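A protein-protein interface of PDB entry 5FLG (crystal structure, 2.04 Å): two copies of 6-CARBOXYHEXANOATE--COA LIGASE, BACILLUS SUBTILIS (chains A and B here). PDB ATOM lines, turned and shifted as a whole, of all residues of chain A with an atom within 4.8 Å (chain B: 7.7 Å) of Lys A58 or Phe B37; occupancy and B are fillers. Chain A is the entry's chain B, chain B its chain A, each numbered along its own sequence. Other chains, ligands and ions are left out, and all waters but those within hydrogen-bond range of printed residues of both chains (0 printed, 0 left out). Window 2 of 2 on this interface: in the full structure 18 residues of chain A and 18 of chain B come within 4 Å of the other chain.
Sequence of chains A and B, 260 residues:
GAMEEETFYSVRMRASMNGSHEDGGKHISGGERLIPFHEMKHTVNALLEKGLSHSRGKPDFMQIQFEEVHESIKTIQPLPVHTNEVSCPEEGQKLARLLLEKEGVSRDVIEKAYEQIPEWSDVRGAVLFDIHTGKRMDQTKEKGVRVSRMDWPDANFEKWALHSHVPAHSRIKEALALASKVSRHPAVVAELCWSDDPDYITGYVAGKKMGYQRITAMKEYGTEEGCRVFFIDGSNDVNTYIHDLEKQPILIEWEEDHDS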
ATOM      1  N   MET A  17      22.601  13.181 -22.978  1.00  0.00           N
ATOM      2  CA  MET A  17      23.170  14.520 -22.978  1.00  0.00           C
ATOM      3  C   MET A  17      24.680  14.508 -22.856  1.00  0.00           C
ATOM      4  O   MET A  17      25.261  13.497 -22.422  1.00  0.00           O
ATOM      5  CB  MET A  17      22.521  15.414 -21.928  1.00  0.00           C
ATOM      6  CG  MET A  17      22.753  15.034 -20.487  1.00  0.00           C
ATOM      7  SD  MET A  17      22.016  16.277 -19.389  1.00  0.00           S
ATOM      8  CE  MET A  17      23.400  17.402 -19.224  1.00  0.00           C
ATOM      9  N   ILE A  28      19.719   9.805 -20.958  1.00  0.00           N
ATOM     10  CA  ILE A  28      18.541  10.494 -20.452  1.00  0.00           C
ATOM     11  C   ILE A  28      17.347   9.544 -20.438  1.00  0.00           C
ATOM     12  O   ILE A  28      16.702   9.399 -19.407  1.00  0.00           O
ATOM     13  CB  ILE A  28      18.197  11.732 -21.285  1.00  0.00           C
ATOM     14  CG1 ILE A  28      19.337  12.754 -21.234  1.00  0.00           C
ATOM     15  CG2 ILE A  28      16.888  12.380 -20.824  1.00  0.00           C
ATOM     16  CD1 ILE A  28      19.453  13.467 -19.917  1.00  0.00           C
ATOM     17  N   LEU A  52      12.153  14.287 -24.629  1.00  0.00           N
ATOM     18  CA  LEU A  52      12.375  15.730 -24.484  1.00  0.00           C
ATOM     19  C   LEU A  52      11.924  16.309 -23.139  1.00  0.00           C
ATOM     20  O   LEU A  52      12.354  17.387 -22.765  1.00  0.00           O
ATOM     21  CB  LEU A  52      11.701  16.512 -25.615  1.00  0.00           C
ATOM     22  CG  LEU A  52      12.155  16.264 -27.035  1.00  0.00           C
ATOM     23  CD1 LEU A  52      11.381  17.145 -27.997  1.00  0.00           C
ATOM     24  CD2 LEU A  52      13.648  16.490 -27.184  1.00  0.00           C
ATOM     25  N   ARG A  56      15.686  13.747 -15.972  1.00  0.00           N
ATOM     26  CA  ARG A  56      17.152  13.639 -15.924  1.00  0.00           C
ATOM     27  C   ARG A  56      17.811  14.737 -16.748  1.00  0.00           C
ATOM     28  O   ARG A  56      19.033  14.837 -16.789  1.00  0.00           O
ATOM     29  CB  ARG A  56      17.616  12.242 -16.404  1.00  0.00           C
ATOM     30  CG  ARG A  56      17.321  11.137 -15.404  1.00  0.00           C
ATOM     31  CD  ARG A  56      17.515   9.732 -15.938  1.00  0.00           C
ATOM     32  NE  ARG A  56      18.869   9.507 -16.431  1.00  0.00           N
ATOM     33  CZ  ARG A  56      19.896   9.105 -15.690  1.00  0.00           C
ATOM     34  NH1 ARG A  56      19.769   8.934 -14.389  1.00  0.00           N
ATOM     35  NH2 ARG A  56      21.071   8.890 -16.253  1.00  0.00           N
ATOM     36  N   GLY A  57      16.997  15.492 -17.476  1.00  0.00           N
ATOM     37  CA  GLY A  57      17.471  16.670 -18.193  1.00  0.00           C
ATOM     38  C   GLY A  57      17.147  16.618 -19.676  1.00  0.00           C
ATOM     39  O   GLY A  57      16.515  15.679 -20.164  1.00  0.00           O
ATOM     40  N   LYS A  58      17.628  17.616 -20.399  1.00  0.00           N
ATOM     41  CA  LYS A  58      17.277  17.800 -21.796  1.00  0.00           C
ATOM     42  C   LYS A  58      18.356  17.147 -22.658  1.00  0.00           C
ATOM     43  O   LYS A  58      19.548  17.320 -22.401  1.00  0.00           O
ATOM     44  CB  LYS A  58      17.154  19.302 -22.081  1.00  0.00           C
ATOM     45  CG  LYS A  58      17.362  19.755 -23.518  1.00  0.00           C
ATOM     46  CD  LYS A  58      17.279  21.278 -23.605  1.00  0.00           C
ATOM     47  CE  LYS A  58      18.028  21.821 -24.813  1.00  0.00           C
ATOM     48  NZ  LYS A  58      17.668  23.244 -25.077  1.00  0.00           N
ATOM     49  N   PRO A  59      17.943  16.281 -23.597  1.00  0.00           N
ATOM     50  CA  PRO A  59      18.940  15.600 -24.430  1.00  0.00           C
ATOM     51  C   PRO A  59      19.521  16.533 -25.475  1.00  0.00           C
ATOM     52  O   PRO A  59      18.831  17.420 -25.915  1.00  0.00           O
ATOM     53  CB  PRO A  59      18.148  14.471 -25.089  1.00  0.00           C
ATOM     54  CG  PRO A  59      16.737  14.931 -25.061  1.00  0.00           C
ATOM     55  CD  PRO A  59      16.573  15.804 -23.848  1.00  0.00           C
ATOM     56  N   ASP A  60      20.789  16.343 -25.834  1.00  0.00           N
ATOM     57  CA  ASP A  60      21.314  16.925 -27.062  1.00  0.00           C
ATOM     58  C   ASP A  60      21.563  15.883 -28.158  1.00  0.00           C
ATOM     59  O   ASP A  60      22.060  16.234 -29.223  1.00  0.00           O
ATOM     60  CB  ASP A  60      22.609  17.724 -26.806  1.00  0.00           C
ATOM     61  CG  ASP A  60      23.651  16.926 -26.079  1.00  0.00           C
ATOM     62  OD1 ASP A  60      23.901  15.752 -26.431  1.00  0.00           O
ATOM     63  OD2 ASP A  60      24.116  17.427 -25.039  1.00  0.00           O
ATOM     64  N   GLU B   6      23.270  31.158 -30.894  1.00  0.00           N
ATOM     65  CA  GLU B   6      22.231  30.141 -30.751  1.00  0.00           C
ATOM     66  C   GLU B   6      22.740  28.730 -31.073  1.00  0.00           C
ATOM     67  O   GLU B   6      23.562  28.539 -31.967  1.00  0.00           O
ATOM     68  CB  GLU B   6      21.040  30.465 -31.639  1.00  0.00           C
ATOM     69  CG  GLU B   6      19.807  29.643 -31.299  1.00  0.00           C
ATOM     70  CD  GLU B   6      18.568  30.105 -32.053  1.00  0.00           C
ATOM     71  OE1 GLU B   6      18.714  30.737 -33.120  1.00  0.00           O
ATOM     72  OE2 GLU B   6      17.442  29.848 -31.565  1.00  0.00           O
ATOM     73  N   THR B   7      22.266  27.749 -30.316  1.00  0.00           N
ATOM     74  CA  THR B   7      22.663  26.361 -30.528  1.00  0.00           C
ATOM     75  C   THR B   7      21.829  25.692 -31.606  1.00  0.00           C
ATOM     76  O   THR B   7      20.587  25.725 -31.563  1.00  0.00           O
ATOM     77  CB  THR B   7      22.586  25.571 -29.221  1.00  0.00           C
ATOM     78  OG1 THR B   7      23.472  26.168 -28.269  1.00  0.00           O
ATOM     79  CG2 THR B   7      23.005  24.118 -29.431  1.00  0.00           C
ATOM     80  N   PHE B   8      22.514  25.073 -32.562  1.00  0.00           N
ATOM     81  CA  PHE B   8      21.858  24.360 -33.639  1.00  0.00           C
ATOM     82  C   PHE B   8      22.028  22.841 -33.567  1.00  0.00           C
ATOM     83  O   PHE B   8      22.920  22.321 -32.877  1.00  0.00           O
ATOM     84  CB  PHE B   8      22.312  24.882 -34.991  1.00  0.00           C
ATOM     85  CG  PHE B   8      21.651  26.170 -35.398  1.00  0.00           C
ATOM     86  CD1 PHE B   8      22.120  27.387 -34.939  1.00  0.00           C
ATOM     87  CD2 PHE B   8      20.559  26.158 -36.264  1.00  0.00           C
ATOM     88  CE1 PHE B   8      21.458  28.569 -35.264  1.00  0.00           C
ATOM     89  CE2 PHE B   8      19.891  27.329 -36.590  1.00  0.00           C
ATOM     90  CZ  PHE B   8      20.309  28.535 -36.048  1.00  0.00           C
ATOM     91  N   TYR B   9      21.048  22.145 -34.160  1.00  0.00           N
ATOM     92  CA  TYR B   9      20.970  20.693 -34.106  1.00  0.00           C
ATOM     93  C   TYR B   9      20.844  20.128 -35.494  1.00  0.00           C
ATOM     94  O   TYR B   9      20.094  20.648 -36.311  1.00  0.00           O
ATOM     95  CB  TYR B   9      19.774  20.247 -33.251  1.00  0.00           C
ATOM     96  CG  TYR B   9      19.914  20.609 -31.802  1.00  0.00           C
ATOM     97  CD1 TYR B   9      19.684  21.898 -31.381  1.00  0.00           C
ATOM     98  CD2 TYR B   9      20.358  19.686 -30.875  1.00  0.00           C
ATOM     99  CE1 TYR B   9      19.857  22.273 -30.071  1.00  0.00           C
ATOM    100  CE2 TYR B   9      20.502  20.035 -29.543  1.00  0.00           C
ATOM    101  CZ  TYR B   9      20.284  21.334 -29.160  1.00  0.00           C
ATOM    102  OH  TYR B   9      20.485  21.734 -27.871  1.00  0.00           O
ATOM    103  N   ILE B  35      18.711  23.066 -37.275  1.00  0.00           N
ATOM    104  CA  ILE B  35      17.641  23.818 -36.647  1.00  0.00           C
ATOM    105  C   ILE B  35      17.927  24.150 -35.202  1.00  0.00           C
ATOM    106  O   ILE B  35      18.698  23.466 -34.532  1.00  0.00           O
ATOM    107  CB  ILE B  35      16.317  23.020 -36.659  1.00  0.00           C
ATOM    108  CG1 ILE B  35      16.548  21.639 -36.039  1.00  0.00           C
ATOM    109  CG2 ILE B  35      15.780  22.923 -38.077  1.00  0.00           C
ATOM    110  CD1 ILE B  35      15.305  21.084 -35.338  1.00  0.00           C
ATOM    111  N   PRO B  36      17.351  25.260 -34.732  1.00  0.00           N
ATOM    112  CA  PRO B  36      17.273  25.475 -33.304  1.00  0.00           C
ATOM    113  C   PRO B  36      16.349  24.485 -32.611  1.00  0.00           C
ATOM    114  O   PRO B  36      15.480  23.890 -33.259  1.00  0.00           O
ATOM    115  CB  PRO B  36      16.706  26.893 -33.184  1.00  0.00           C
ATOM    116  CG  PRO B  36      16.124  27.214 -34.502  1.00  0.00           C
ATOM    117  CD  PRO B  36      16.510  26.182 -35.502  1.00  0.00           C
ATOM    118  N   PHE B  37      16.487  24.385 -31.298  1.00  0.00           N
ATOM    119  CA  PHE B  37      15.942  23.290 -30.578  1.00  0.00           C
ATOM    120  C   PHE B  37      14.411  23.372 -30.526  1.00  0.00           C
ATOM    121  O   PHE B  37      13.744  22.353 -30.438  1.00  0.00           O
ATOM    122  CB  PHE B  37      16.503  23.263 -29.164  1.00  0.00           C
ATOM    123  CG  PHE B  37      16.136  22.011 -28.399  1.00  0.00           C
ATOM    124  CD1 PHE B  37      16.802  20.824 -28.637  1.00  0.00           C
ATOM    125  CD2 PHE B  37      15.092  22.027 -27.481  1.00  0.00           C
ATOM    126  CE1 PHE B  37      16.475  19.682 -27.926  1.00  0.00           C
ATOM    127  CE2 PHE B  37      14.757  20.894 -26.775  1.00  0.00           C
ATOM    128  CZ  PHE B  37      15.443  19.720 -27.002  1.00  0.00           C
ATOM    129  N   HIS B  38      13.872  24.583 -30.574  1.00  0.00           N
ATOM    130  CA  HIS B  38      12.427  24.753 -30.500  1.00  0.00           C
ATOM    131  C   HIS B  38      11.786  24.343 -31.817  1.00  0.00           C
ATOM    132  O   HIS B  38      10.570  24.178 -31.898  1.00  0.00           O
ATOM    133  CB  HIS B  38      12.066  26.198 -30.159  1.00  0.00           C
ATOM    134  CG  HIS B  38      12.601  27.208 -31.129  1.00  0.00           C
ATOM    135  ND1 HIS B  38      11.960  27.527 -32.306  1.00  0.00           N
ATOM    136  CD2 HIS B  38      13.717  27.973 -31.088  1.00  0.00           C
ATOM    137  CE1 HIS B  38      12.644  28.461 -32.938  1.00  0.00           C
ATOM    138  NE2 HIS B  38      13.688  28.784 -32.194  1.00  0.00           N
ATOM    139  N   GLU B  39      12.589  24.058 -32.839  1.00  0.00           N
ATOM    140  CA  GLU B  39      11.971  23.525 -34.046  1.00  0.00           C
ATOM    141  C   GLU B  39      11.946  21.997 -34.149  1.00  0.00           C
ATOM    142  O   GLU B  39      11.513  21.443 -35.149  1.00  0.00           O
ATOM    143  CB  GLU B  39      12.553  24.175 -35.284  1.00  0.00           C
ATOM    144  CG  GLU B  39      12.095  25.608 -35.485  1.00  0.00           C
ATOM    145  CD  GLU B  39      12.845  26.317 -36.603  1.00  0.00           C
ATOM    146  OE1 GLU B  39      13.154  25.675 -37.626  1.00  0.00           O
ATOM    147  OE2 GLU B  39      13.020  27.545 -36.512  1.00  0.00           O
ATOM    148  N   MET B  40      12.291  21.317 -33.076  1.00  0.00           N
ATOM    149  CA  MET B  40      12.568  19.891 -33.153  1.00  0.00           C
ATOM    150  C   MET B  40      11.285  19.092 -33.464  1.00  0.00           C
ATOM    151  O   MET B  40      11.291  18.158 -34.290  1.00  0.00           O
ATOM    152  CB  MET B  40      13.179  19.426 -31.848  1.00  0.00           C
ATOM    153  CG  MET B  40      13.740  18.012 -31.899  1.00  0.00           C
ATOM    154  SD  MET B  40      14.930  17.730 -33.228  1.00  0.00           S
ATOM    155  CE  MET B  40      16.379  18.495 -32.474  1.00  0.00           C
ATOM    156  N   LYS B  41      10.185  19.442 -32.814  1.00  0.00           N
ATOM    157  CA  LYS B  41       8.986  18.615 -32.965  1.00  0.00           C
ATOM    158  C   LYS B  41       8.475  18.682 -34.380  1.00  0.00           C
ATOM    159  O   LYS B  41       8.190  17.664 -34.997  1.00  0.00           O
ATOM    160  CB  LYS B  41       7.888  19.052 -32.004  1.00  0.00           C
ATOM    161  CG  LYS B  41       6.593  18.276 -32.202  1.00  0.00           C
ATOM    162  CD  LYS B  41       5.633  18.403 -31.026  1.00  0.00           C
ATOM    163  CE  LYS B  41       4.379  19.172 -31.426  1.00  0.00           C
ATOM    164  NZ  LYS B  41       3.610  18.436 -32.463  1.00  0.00           N
ATOM    165  N   HIS B  42       8.420  19.886 -34.922  1.00  0.00           N
ATOM    166  CA  HIS B  42       7.997  20.084 -36.297  1.00  0.00           C
ATOM    167  C   HIS B  42       8.932  19.413 -37.277  1.00  0.00           C
ATOM    168  O   HIS B  42       8.512  18.966 -38.325  1.00  0.00           O
ATOM    169  CB  HIS B  42       7.910  21.586 -36.589  1.00  0.00           C
ATOM    170  CG  HIS B  42       7.682  21.921 -38.033  1.00  0.00           C
ATOM    171  ND1 HIS B  42       6.421  21.979 -38.597  1.00  0.00           N
ATOM    172  CD2 HIS B  42       8.548  22.265 -39.019  1.00  0.00           C
ATOM    173  CE1 HIS B  42       6.532  22.248 -39.887  1.00  0.00           C
ATOM    174  NE2 HIS B  42       7.811  22.428 -40.169  1.00  0.00           N
ATOM    175  N   THR B  43      10.232  19.425 -36.990  1.00  0.00           N
ATOM    176  CA  THR B  43      11.215  18.972 -37.963  1.00  0.00           C
ATOM    177  C   THR B  43      11.262  17.455 -37.997  1.00  0.00           C
ATOM    178  O   THR B  43      11.243  16.863 -39.045  1.00  0.00           O
ATOM    179  CB  THR B  43      12.601  19.466 -37.573  1.00  0.00           C
ATOM    180  OG1 THR B  43      12.627  20.888 -37.649  1.00  0.00           O
ATOM    181  CG2 THR B  43      13.669  18.899 -38.489  1.00  0.00           C
ATOM    182  N   PHE B  66      18.961  13.227 -33.999  1.00  0.00           N
ATOM    183  CA  PHE B  66      19.437  14.582 -33.837  1.00  0.00           C
ATOM    184  C   PHE B  66      20.614  14.660 -32.908  1.00  0.00           C
ATOM    185  O   PHE B  66      20.789  13.809 -32.042  1.00  0.00           O
ATOM    186  CB  PHE B  66      18.312  15.562 -33.422  1.00  0.00           C
ATOM    187  CG  PHE B  66      17.919  15.486 -31.990  1.00  0.00           C
ATOM    188  CD1 PHE B  66      18.757  15.976 -31.003  1.00  0.00           C
ATOM    189  CD2 PHE B  66      16.603  15.140 -31.644  1.00  0.00           C
ATOM    190  CE1 PHE B  66      18.369  15.944 -29.674  1.00  0.00           C
ATOM    191  CE2 PHE B  66      16.169  15.227 -30.333  1.00  0.00           C
ATOM    192  CZ  PHE B  66      17.049  15.627 -29.341  1.00  0.00           C
ATOM    193  N   GLU B  68      23.442  17.854 -31.286  1.00  0.00           N
ATOM    194  CA  GLU B  68      24.013  19.168 -31.197  1.00  0.00           C
ATOM    195  C   GLU B  68      25.196  19.331 -32.127  1.00  0.00           C
ATOM    196  O   GLU B  68      26.075  18.477 -32.195  1.00  0.00           O
ATOM    197  CB  GLU B  68      24.475  19.413 -29.762  1.00  0.00           C
ATOM    198  CG  GLU B  68      24.829  20.853 -29.476  1.00  0.00           C
ATOM    199  CD  GLU B  68      25.178  21.088 -28.012  1.00  0.00           C
ATOM    200  OE1 GLU B  68      25.092  20.150 -27.183  1.00  0.00           O
ATOM    201  OE2 GLU B  68      25.420  22.252 -27.680  1.00  0.00           O
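Of the 8 printed residues of chain A, 4 touch a printed residue of chain B. Printed residues of chain B that touch a printed residue of chain A: Tyr B9, Phe B37, Phe B66 and Glu B68. Among the printed residues, 6 pairs touch across the chains. Among the printed residues, no Asp or Glu carboxylate lies within 4 Å of a Lys or Arg side-chain nitrogen of the other chain.
Phe B37 touches Leu A52 (CZ to CD2, 3.7 Å). Tyr B9 touches Lys A58. Phe B37 touches Lys A58 (CD2 to NZ, 3.7 Å). Pro A59 touches Phe B37 (O to CE1, 3.8 Å). Phe B66 touches Asp A60.
Of chain B, only Tyr B9 (3.9 Å) and Phe B37 (3.7 Å) come within 4 Å of Lys A58. Pro A59 touches one residue of chain B. Of the printed residues of chain A, Tyr B9 touches Lys A58 (3.9 Å). Of the printed residues of chain B, Asp A60 touches Phe B66 and Glu B68. Printed residues of chain B within 4 Å of Leu A52: Phe B37. Printed residues of chain A within 4 Å of Phe B66: Asp A60 (3.5 Å). Met B40 touches none of the printed residues of chain A. The nearest printed residue of chain B that does not touch Lys A58 is His B38 (6.8 Å). The nearest printed residue of chain A that does not touch Glu B68 is Pro A59 (6.9 Å).
No position is printed for both chains.
The backbone NH (N) of Glu B68 is in hydrogen-bond range of the backbone carbonyl oxygen (O) of Asp A60 (3.0 Å).
O of Ile B35 sits at hydrogen-bond distance from N of Tyr B9 (2.7 Å).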
